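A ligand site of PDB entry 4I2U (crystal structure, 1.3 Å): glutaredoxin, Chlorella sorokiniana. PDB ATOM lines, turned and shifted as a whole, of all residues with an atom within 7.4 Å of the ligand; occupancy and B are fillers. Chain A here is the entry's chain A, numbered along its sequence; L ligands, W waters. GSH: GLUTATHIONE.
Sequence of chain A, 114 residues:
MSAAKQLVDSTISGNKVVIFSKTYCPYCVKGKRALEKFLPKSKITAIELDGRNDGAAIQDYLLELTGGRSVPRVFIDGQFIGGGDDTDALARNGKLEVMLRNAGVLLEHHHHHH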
ATOM      1  N   LYS A  22     -11.815  30.417   6.985  1.00  0.00           N
ATOM      2  CA  LYS A  22     -12.954  30.934   7.752  1.00  0.00           C
ATOM      3  C   LYS A  22     -13.824  29.759   8.111  1.00  0.00           C
ATOM      4  O   LYS A  22     -13.976  28.812   7.338  1.00  0.00           O
ATOM      5  CB  LYS A  22     -13.740  31.988   6.980  1.00  0.00           C
ATOM      6  CG  LYS A  22     -12.939  33.253   6.812  1.00  0.00           C
ATOM      7  CD  LYS A  22     -13.616  34.332   6.017  1.00  0.00           C
ATOM      8  CE  LYS A  22     -12.684  35.508   5.810  1.00  0.00           C
ATOM      9  NZ  LYS A  22     -13.340  36.606   5.083  1.00  0.00           N
ATOM     10  N   TYR A  24     -16.906  29.057   8.352  1.00  0.00           N
ATOM     11  CA  TYR A  24     -18.162  28.817   7.659  1.00  0.00           C
ATOM     12  C   TYR A  24     -18.009  28.462   6.180  1.00  0.00           C
ATOM     13  O   TYR A  24     -18.993  28.168   5.519  1.00  0.00           O
ATOM     14  CB  TYR A  24     -19.027  30.056   7.774  1.00  0.00           C
ATOM     15  CG  TYR A  24     -18.403  31.336   7.266  1.00  0.00           C
ATOM     16  CD1 TYR A  24     -18.210  31.565   5.910  1.00  0.00           C
ATOM     17  CD2 TYR A  24     -18.020  32.351   8.160  1.00  0.00           C
ATOM     18  CE1 TYR A  24     -17.663  32.746   5.432  1.00  0.00           C
ATOM     19  CE2 TYR A  24     -17.463  33.533   7.682  1.00  0.00           C
ATOM     20  CZ  TYR A  24     -17.309  33.716   6.324  1.00  0.00           C
ATOM     21  OH  TYR A  24     -16.833  34.896   5.793  1.00  0.00           O
ATOM     22  N   CYS A  25     -16.777  28.503   5.677  1.00  0.00           N
ATOM     23  CA  CYS A  25     -16.537  28.353   4.242  1.00  0.00           C
ATOM     24  C   CYS A  25     -16.363  26.891   3.823  1.00  0.00           C
ATOM     25  O   CYS A  25     -15.538  26.175   4.388  1.00  0.00           O
ATOM     26  CB  CYS A  25     -15.269  29.128   3.885  1.00  0.00           C
ATOM     27  SG  CYS A  25     -14.608  28.778   2.227  1.00  0.00           S
ATOM     28  N   PRO A  26     -17.139  26.440   2.825  1.00  0.00           N
ATOM     29  CA  PRO A  26     -17.026  25.044   2.412  1.00  0.00           C
ATOM     30  C   PRO A  26     -15.730  24.706   1.699  1.00  0.00           C
ATOM     31  O   PRO A  26     -15.316  23.563   1.687  1.00  0.00           O
ATOM     32  CB  PRO A  26     -18.218  24.854   1.470  1.00  0.00           C
ATOM     33  CG  PRO A  26     -18.477  26.253   0.918  1.00  0.00           C
ATOM     34  CD  PRO A  26     -18.207  27.163   2.085  1.00  0.00           C
ATOM     35  N   TYR A  27     -15.071  25.708   1.122  1.00  0.00           N
ATOM     36  CA  TYR A  27     -13.766  25.481   0.492  1.00  0.00           C
ATOM     37  C   TYR A  27     -12.713  25.265   1.561  1.00  0.00           C
ATOM     38  O   TYR A  27     -11.798  24.454   1.375  1.00  0.00           O
ATOM     39  CB  TYR A  27     -13.426  26.628  -0.469  1.00  0.00           C
ATOM     40  CG  TYR A  27     -14.345  26.604  -1.656  1.00  0.00           C
ATOM     41  CD1 TYR A  27     -14.075  25.804  -2.754  1.00  0.00           C
ATOM     42  CD2 TYR A  27     -15.521  27.329  -1.659  1.00  0.00           C
ATOM     43  CE1 TYR A  27     -14.922  25.738  -3.837  1.00  0.00           C
ATOM     44  CE2 TYR A  27     -16.387  27.262  -2.741  1.00  0.00           C
ATOM     45  CZ  TYR A  27     -16.078  26.480  -3.825  1.00  0.00           C
ATOM     46  OH  TYR A  27     -16.954  26.438  -4.875  1.00  0.00           O
ATOM     47  N   CYS A  28     -12.830  25.978   2.673  1.00  0.00           N
ATOM     48  CA  CYS A  28     -11.957  25.757   3.822  1.00  0.00           C
ATOM     49  C   CYS A  28     -12.188  24.382   4.412  1.00  0.00           C
ATOM     50  O   CYS A  28     -11.227  23.655   4.709  1.00  0.00           O
ATOM     51  CB  CYS A  28     -12.184  26.862   4.868  1.00  0.00           C
ATOM     52  SG  CYS A  28     -11.678  28.468   4.266  1.00  0.00           S
ATOM     53  N   LYS A  30     -13.309  21.804   2.790  1.00  0.00           N
ATOM     54  CA  LYS A  30     -12.775  20.873   1.799  1.00  0.00           C
ATOM     55  C   LYS A  30     -11.240  20.757   1.913  1.00  0.00           C
ATOM     56  O   LYS A  30     -10.678  19.667   1.835  1.00  0.00           O
ATOM     57  CB  LYS A  30     -13.168  21.348   0.399  1.00  0.00           C
ATOM     58  CG  LYS A  30     -12.659  20.521  -0.754  1.00  0.00           C
ATOM     59  CD  LYS A  30     -12.986  21.205  -2.102  1.00  0.00           C
ATOM     60  CE  LYS A  30     -14.484  21.390  -2.309  1.00  0.00           C
ATOM     61  NZ  LYS A  30     -14.752  21.626  -3.773  1.00  0.00           N
ATOM     62  N   GLN A  59      -6.033  38.887   5.245  1.00  0.00           N
ATOM     63  CA  GLN A  59      -6.410  38.609   3.857  1.00  0.00           C
ATOM     64  C   GLN A  59      -5.746  39.570   2.896  1.00  0.00           C
ATOM     65  O   GLN A  59      -5.355  39.157   1.808  1.00  0.00           O
ATOM     66  CB  GLN A  59      -7.915  38.671   3.668  1.00  0.00           C
ATOM     67  CG  GLN A  59      -8.660  37.539   4.355  1.00  0.00           C
ATOM     68  CD  GLN A  59     -10.146  37.548   4.036  1.00  0.00           C
ATOM     69  OE1 GLN A  59     -10.965  38.090   4.791  1.00  0.00           O
ATOM     70  NE2 GLN A  59     -10.512  36.994   2.894  1.00  0.00           N
ATOM     71  N   ARG A  69      -7.217  37.053  -2.284  1.00  0.00           N
ATOM     72  CA  ARG A  69      -7.679  37.266  -0.917  1.00  0.00           C
ATOM     73  C   ARG A  69      -8.567  36.155  -0.401  1.00  0.00           C
ATOM     74  O   ARG A  69      -8.796  36.079   0.804  1.00  0.00           O
ATOM     75  CB  ARG A  69      -8.545  38.530  -0.844  1.00  0.00           C
ATOM     76  CG  ARG A  69      -7.847  39.807  -0.485  1.00  0.00           C
ATOM     77  CD  ARG A  69      -8.848  40.934  -0.289  1.00  0.00           C
ATOM     78  NE  ARG A  69      -8.828  41.490   1.061  1.00  0.00           N
ATOM     79  CZ  ARG A  69      -9.811  41.361   1.957  1.00  0.00           C
ATOM     80  NH1 ARG A  69     -10.901  40.654   1.665  1.00  0.00           N
ATOM     81  NH2 ARG A  69      -9.704  41.925   3.140  1.00  0.00           N
ATOM     82  N   SER A  70      -9.104  35.334  -1.289  1.00  0.00           N
ATOM     83  CA  SER A  70     -10.138  34.380  -0.881  1.00  0.00           C
ATOM     84  C   SER A  70      -9.569  33.345   0.080  1.00  0.00           C
ATOM     85  O   SER A  70      -8.383  33.063   0.103  1.00  0.00           O
ATOM     86  CB  SER A  70     -10.722  33.673  -2.088  1.00  0.00           C
ATOM     87  OG  SER A  70      -9.776  32.873  -2.768  1.00  0.00           O
ATOM     88  N   VAL A  71     -10.454  32.767   0.882  1.00  0.00           N
ATOM     89  CA  VAL A  71     -10.106  31.641   1.742  1.00  0.00           C
ATOM     90  C   VAL A  71     -10.618  30.353   1.137  1.00  0.00           C
ATOM     91  O   VAL A  71     -11.668  30.320   0.507  1.00  0.00           O
ATOM     92  CB  VAL A  71     -10.626  31.798   3.187  1.00  0.00           C
ATOM     93  CG1 VAL A  71      -9.890  32.943   3.851  1.00  0.00           C
ATOM     94  CG2 VAL A  71     -12.141  32.030   3.220  1.00  0.00           C
ATOM     95  N   PRO A  72      -9.892  29.253   1.311  1.00  0.00           N
ATOM     96  CA  PRO A  72      -8.647  29.182   2.091  1.00  0.00           C
ATOM     97  C   PRO A  72      -7.408  29.552   1.287  1.00  0.00           C
ATOM     98  O   PRO A  72      -7.429  29.615   0.067  1.00  0.00           O
ATOM     99  CB  PRO A  72      -8.569  27.696   2.475  1.00  0.00           C
ATOM    100  CG  PRO A  72      -9.214  27.020   1.267  1.00  0.00           C
ATOM    101  CD  PRO A  72     -10.351  27.924   0.863  1.00  0.00           C
ATOM    102  N   ARG A  73      -6.310  29.777   2.008  1.00  0.00           N
ATOM    103  CA  ARG A  73      -4.982  29.867   1.408  1.00  0.00           C
ATOM    104  C   ARG A  73      -4.118  28.888   2.170  1.00  0.00           C
ATOM    105  O   ARG A  73      -3.941  28.995   3.371  1.00  0.00           O
ATOM    106  CB  ARG A  73      -4.421  31.286   1.470  1.00  0.00           C
ATOM    107  CG  ARG A  73      -5.305  32.341   0.785  1.00  0.00           C
ATOM    108  CD  ARG A  73      -4.963  32.549  -0.682  1.00  0.00           C
ATOM    109  NE  ARG A  73      -6.105  32.947  -1.492  1.00  0.00           N
ATOM    110  CZ  ARG A  73      -6.022  33.210  -2.785  1.00  0.00           C
ATOM    111  NH1 ARG A  73      -4.851  33.186  -3.412  1.00  0.00           N
ATOM    112  NH2 ARG A  73      -7.120  33.511  -3.467  1.00  0.00           N
ATOM    113  N   GLY A  82      -2.390  26.924  -3.070  1.00  0.00           N
ATOM    114  CA  GLY A  82      -3.697  27.262  -3.625  1.00  0.00           C
ATOM    115  C   GLY A  82      -4.801  27.282  -2.595  1.00  0.00           C
ATOM    116  O   GLY A  82      -4.554  27.378  -1.401  1.00  0.00           O
ATOM    117  N   GLY A  83      -6.019  27.238  -3.110  1.00  0.00           N
ATOM    118  CA  GLY A  83      -7.216  27.248  -2.281  1.00  0.00           C
ATOM    119  C   GLY A  83      -7.782  25.865  -2.023  1.00  0.00           C
ATOM    120  O   GLY A  83      -7.040  24.858  -2.018  1.00  0.00           O
ATOM    121  N   GLY A  84      -9.078  25.800  -1.780  1.00  0.00           N
ATOM    122  CA  GLY A  84      -9.694  24.541  -1.378  1.00  0.00           C
ATOM    123  C   GLY A  84      -9.781  23.525  -2.501  1.00  0.00           C
ATOM    124  O   GLY A  84      -9.442  22.349  -2.303  1.00  0.00           O
ATOM    125  N   ASP A  85     -10.249  23.966  -3.670  1.00  0.00           N
ATOM    126  CA  ASP A  85     -10.289  23.083  -4.817  1.00  0.00           C
ATOM    127  C   ASP A  85      -8.884  22.606  -5.169  1.00  0.00           C
ATOM    128  O   ASP A  85      -8.694  21.441  -5.452  1.00  0.00           O
ATOM    129  CB  ASP A  85     -10.904  23.787  -6.019  1.00  0.00           C
ATOM    130  CG  ASP A  85     -12.406  23.963  -5.887  1.00  0.00           C
ATOM    131  OD1 ASP A  85     -13.038  23.288  -5.046  1.00  0.00           O
ATOM    132  OD2 ASP A  85     -12.916  24.805  -6.638  1.00  0.00           O
ATOM    133  N   ASP A  86      -7.892  23.497  -5.128  1.00  0.00           N
ATOM    134  CA  ASP A  86      -6.518  23.108  -5.451  1.00  0.00           C
ATOM    135  C   ASP A  86      -6.010  22.061  -4.463  1.00  0.00           C
ATOM    136  O   ASP A  86      -5.375  21.075  -4.867  1.00  0.00           O
ATOM    137  CB  ASP A  86      -5.553  24.303  -5.407  1.00  0.00           C
ATOM    138  CG  ASP A  86      -5.842  25.331  -6.454  1.00  0.00           C
ATOM    139  OD1 ASP A  86      -6.243  24.977  -7.582  1.00  0.00           O
ATOM    140  OD2 ASP A  86      -5.623  26.530  -6.145  1.00  0.00           O
ATOM    141  N   THR A  87      -6.254  22.276  -3.185  1.00  0.00           N
ATOM    142  CA  THR A  87      -5.728  21.380  -2.173  1.00  0.00           C
ATOM    143  C   THR A  87      -6.381  20.012  -2.289  1.00  0.00           C
ATOM    144  O   THR A  87      -5.706  18.973  -2.172  1.00  0.00           O
ATOM    145  CB  THR A  87      -5.928  21.977  -0.763  1.00  0.00           C
ATOM    146  OG1 THR A  87      -5.202  23.204  -0.654  1.00  0.00           O
ATOM    147  CG2 THR A  87      -5.420  21.032   0.313  1.00  0.00           C
HETATM  148  N1  GSH L   1     -12.424  28.229  -5.670  1.00  0.00           N
HETATM  149  CA1 GSH L   1     -11.947  28.860  -4.431  1.00  0.00           C
HETATM  150  C1  GSH L   1     -11.202  27.793  -3.663  1.00  0.00           C
HETATM  151  O11 GSH L   1     -11.135  26.653  -4.161  1.00  0.00           O
HETATM  152  O12 GSH L   1     -10.659  28.062  -2.565  1.00  0.00           O
HETATM  153  CB1 GSH L   1     -13.149  29.446  -3.702  1.00  0.00           C
HETATM  154  CG1 GSH L   1     -12.775  30.225  -2.438  1.00  0.00           C
HETATM  155  CD1 GSH L   1     -13.812  31.271  -2.099  1.00  0.00           C
HETATM  156  OE1 GSH L   1     -14.322  31.990  -2.961  1.00  0.00           O
HETATM  157  N2  GSH L   1     -14.114  31.417  -0.824  1.00  0.00           N
HETATM  158  CA2 GSH L   1     -15.020  32.469  -0.348  1.00  0.00           C
HETATM  159  C2  GSH L   1     -14.281  33.743   0.001  1.00  0.00           C
HETATM  160  O2  GSH L   1     -13.068  33.743   0.177  1.00  0.00           O
HETATM  161  CB2 GSH L   1     -15.830  31.974   0.852  1.00  0.00           C
HETATM  162  SG2 GSH L   1     -17.020  30.694   0.389  1.00  0.00           S
HETATM  163  N3  GSH L   1     -14.994  34.858   0.070  1.00  0.00           N
HETATM  164  CA3 GSH L   1     -14.358  36.137   0.256  1.00  0.00           C
HETATM  165  C3  GSH L   1     -13.831  36.386   1.644  1.00  0.00           C
HETATM  166  O31 GSH L   1     -14.150  35.648   2.595  1.00  0.00           O
HETATM  167  O32 GSH L   1     -13.070  37.376   1.754  1.00  0.00           O
HETATM  168  O   HOH W   1     -13.846  32.569  -5.571  1.00  0.00           O
HETATM  169  O   HOH W   2      -9.198  30.355  -1.955  1.00  0.00           O
HETATM  170  O   HOH W   3     -16.583  34.793   3.178  1.00  0.00           O
HETATM  171  O   HOH W   4      -8.432  26.330  -5.087  1.00  0.00           O
HETATM  172  O   HOH W   5     -12.085  38.838  -0.362  1.00  0.00           O
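NZ of Lys 22 is in salt-bridge range of O31 of the ligand (2.8 Å).
The side-chain amide nitrogen (NE2) of Gln 59 is in hydrogen-bond range of an oxygen (O32) of the ligand, 2.8 Å away.
N of Gly 84 sits at hydrogen-bond distance from O12 of the ligand, at 2.9 Å.
N of Asp 85 sits at hydrogen-bond distance from O11 of the ligand (2.9 Å).
A nitrogen (N1) of the ligand lies within salt-bridge range of the side-chain carboxylate (OD2) of Asp 85, at 3.6 Å.
An oxygen (O2) of the ligand is in hydrogen-bond range of the backbone NH (N) of Val 71, 2.9 Å away.
The backbone carbonyl oxygen of Val 71 is in hydrogen-bond range of a nitrogen (N2) of the ligand (3.0 Å).
The side-chain sulfur (SG) of Cys 25 lies close to a sulfur (SG2) of the ligand, 3.6 Å away.
The guanidinium group (NH1) of Arg 69 lies within salt-bridge range of an oxygen (O32) of the ligand (3.9 Å).
The side-chain amino group (NZ) of Lys 22 lies within hydrogen-bond range of the side-chain amide oxygen (OE1) of Gln 59, at 2.8 Å.
The side-chain sulfur of Cys 28 lies within hydrogen-bond range of the backbone NH of Lys 22 (3.3 Å).
The side-chain amide nitrogen of Gln 59 is in hydrogen-bond range of the backbone carbonyl oxygen of Arg 69, 2.9 Å away.
The side-chain carboxylate (OD1) of Asp 85 is in salt-bridge range of the side-chain amino group (NZ) of Lys 30 (2.7 Å).
SG of Cys 25 lies within hydrogen-bond range of O of Val 71, 3.7 Å away.
The backbone carbonyl oxygen of Ser 70 lies within hydrogen-bond range of the guanidinium group of Arg 73, 2.8 Å away.
O of Gly 83 sits at hydrogen-bond distance from OG1 of Thr 87 (2.8 Å).
The side-chain sulfur of Cys 25 is in hydrogen-bond range of the backbone NH of Cys 28 (3.3 Å).
Tyr 27 touches the ligand (CD1 to O11, 3.4 Å).
Ser 70 touches the ligand.
CD of Pro 72 touches O12 of the ligand (3.4 Å).
Gly 83 touches the ligand (CA to O12, 3.5 Å).
Hydrophobic or aromatic side chains that line the ligand: Tyr 27, Val 71 and Pro 72.
Water W3 lies within hydrogen-bond range of the side-chain hydroxyl (OH) of Tyr 24 and an oxygen (O31) of the ligand.
Water W5 lies within hydrogen-bond range of an oxygen (O32) of the ligand and the guanidinium group (NH1) of Arg 69.
Water W2 lies within hydrogen-bond range of the side-chain hydroxyl of Ser 70 (2.7 Å), the backbone carbonyl oxygen of Pro 72 (2.8 Å), an oxygen (O12) of the ligand (2.8 Å) and the backbone carbonyl oxygen of Val 71 (3.5 Å).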
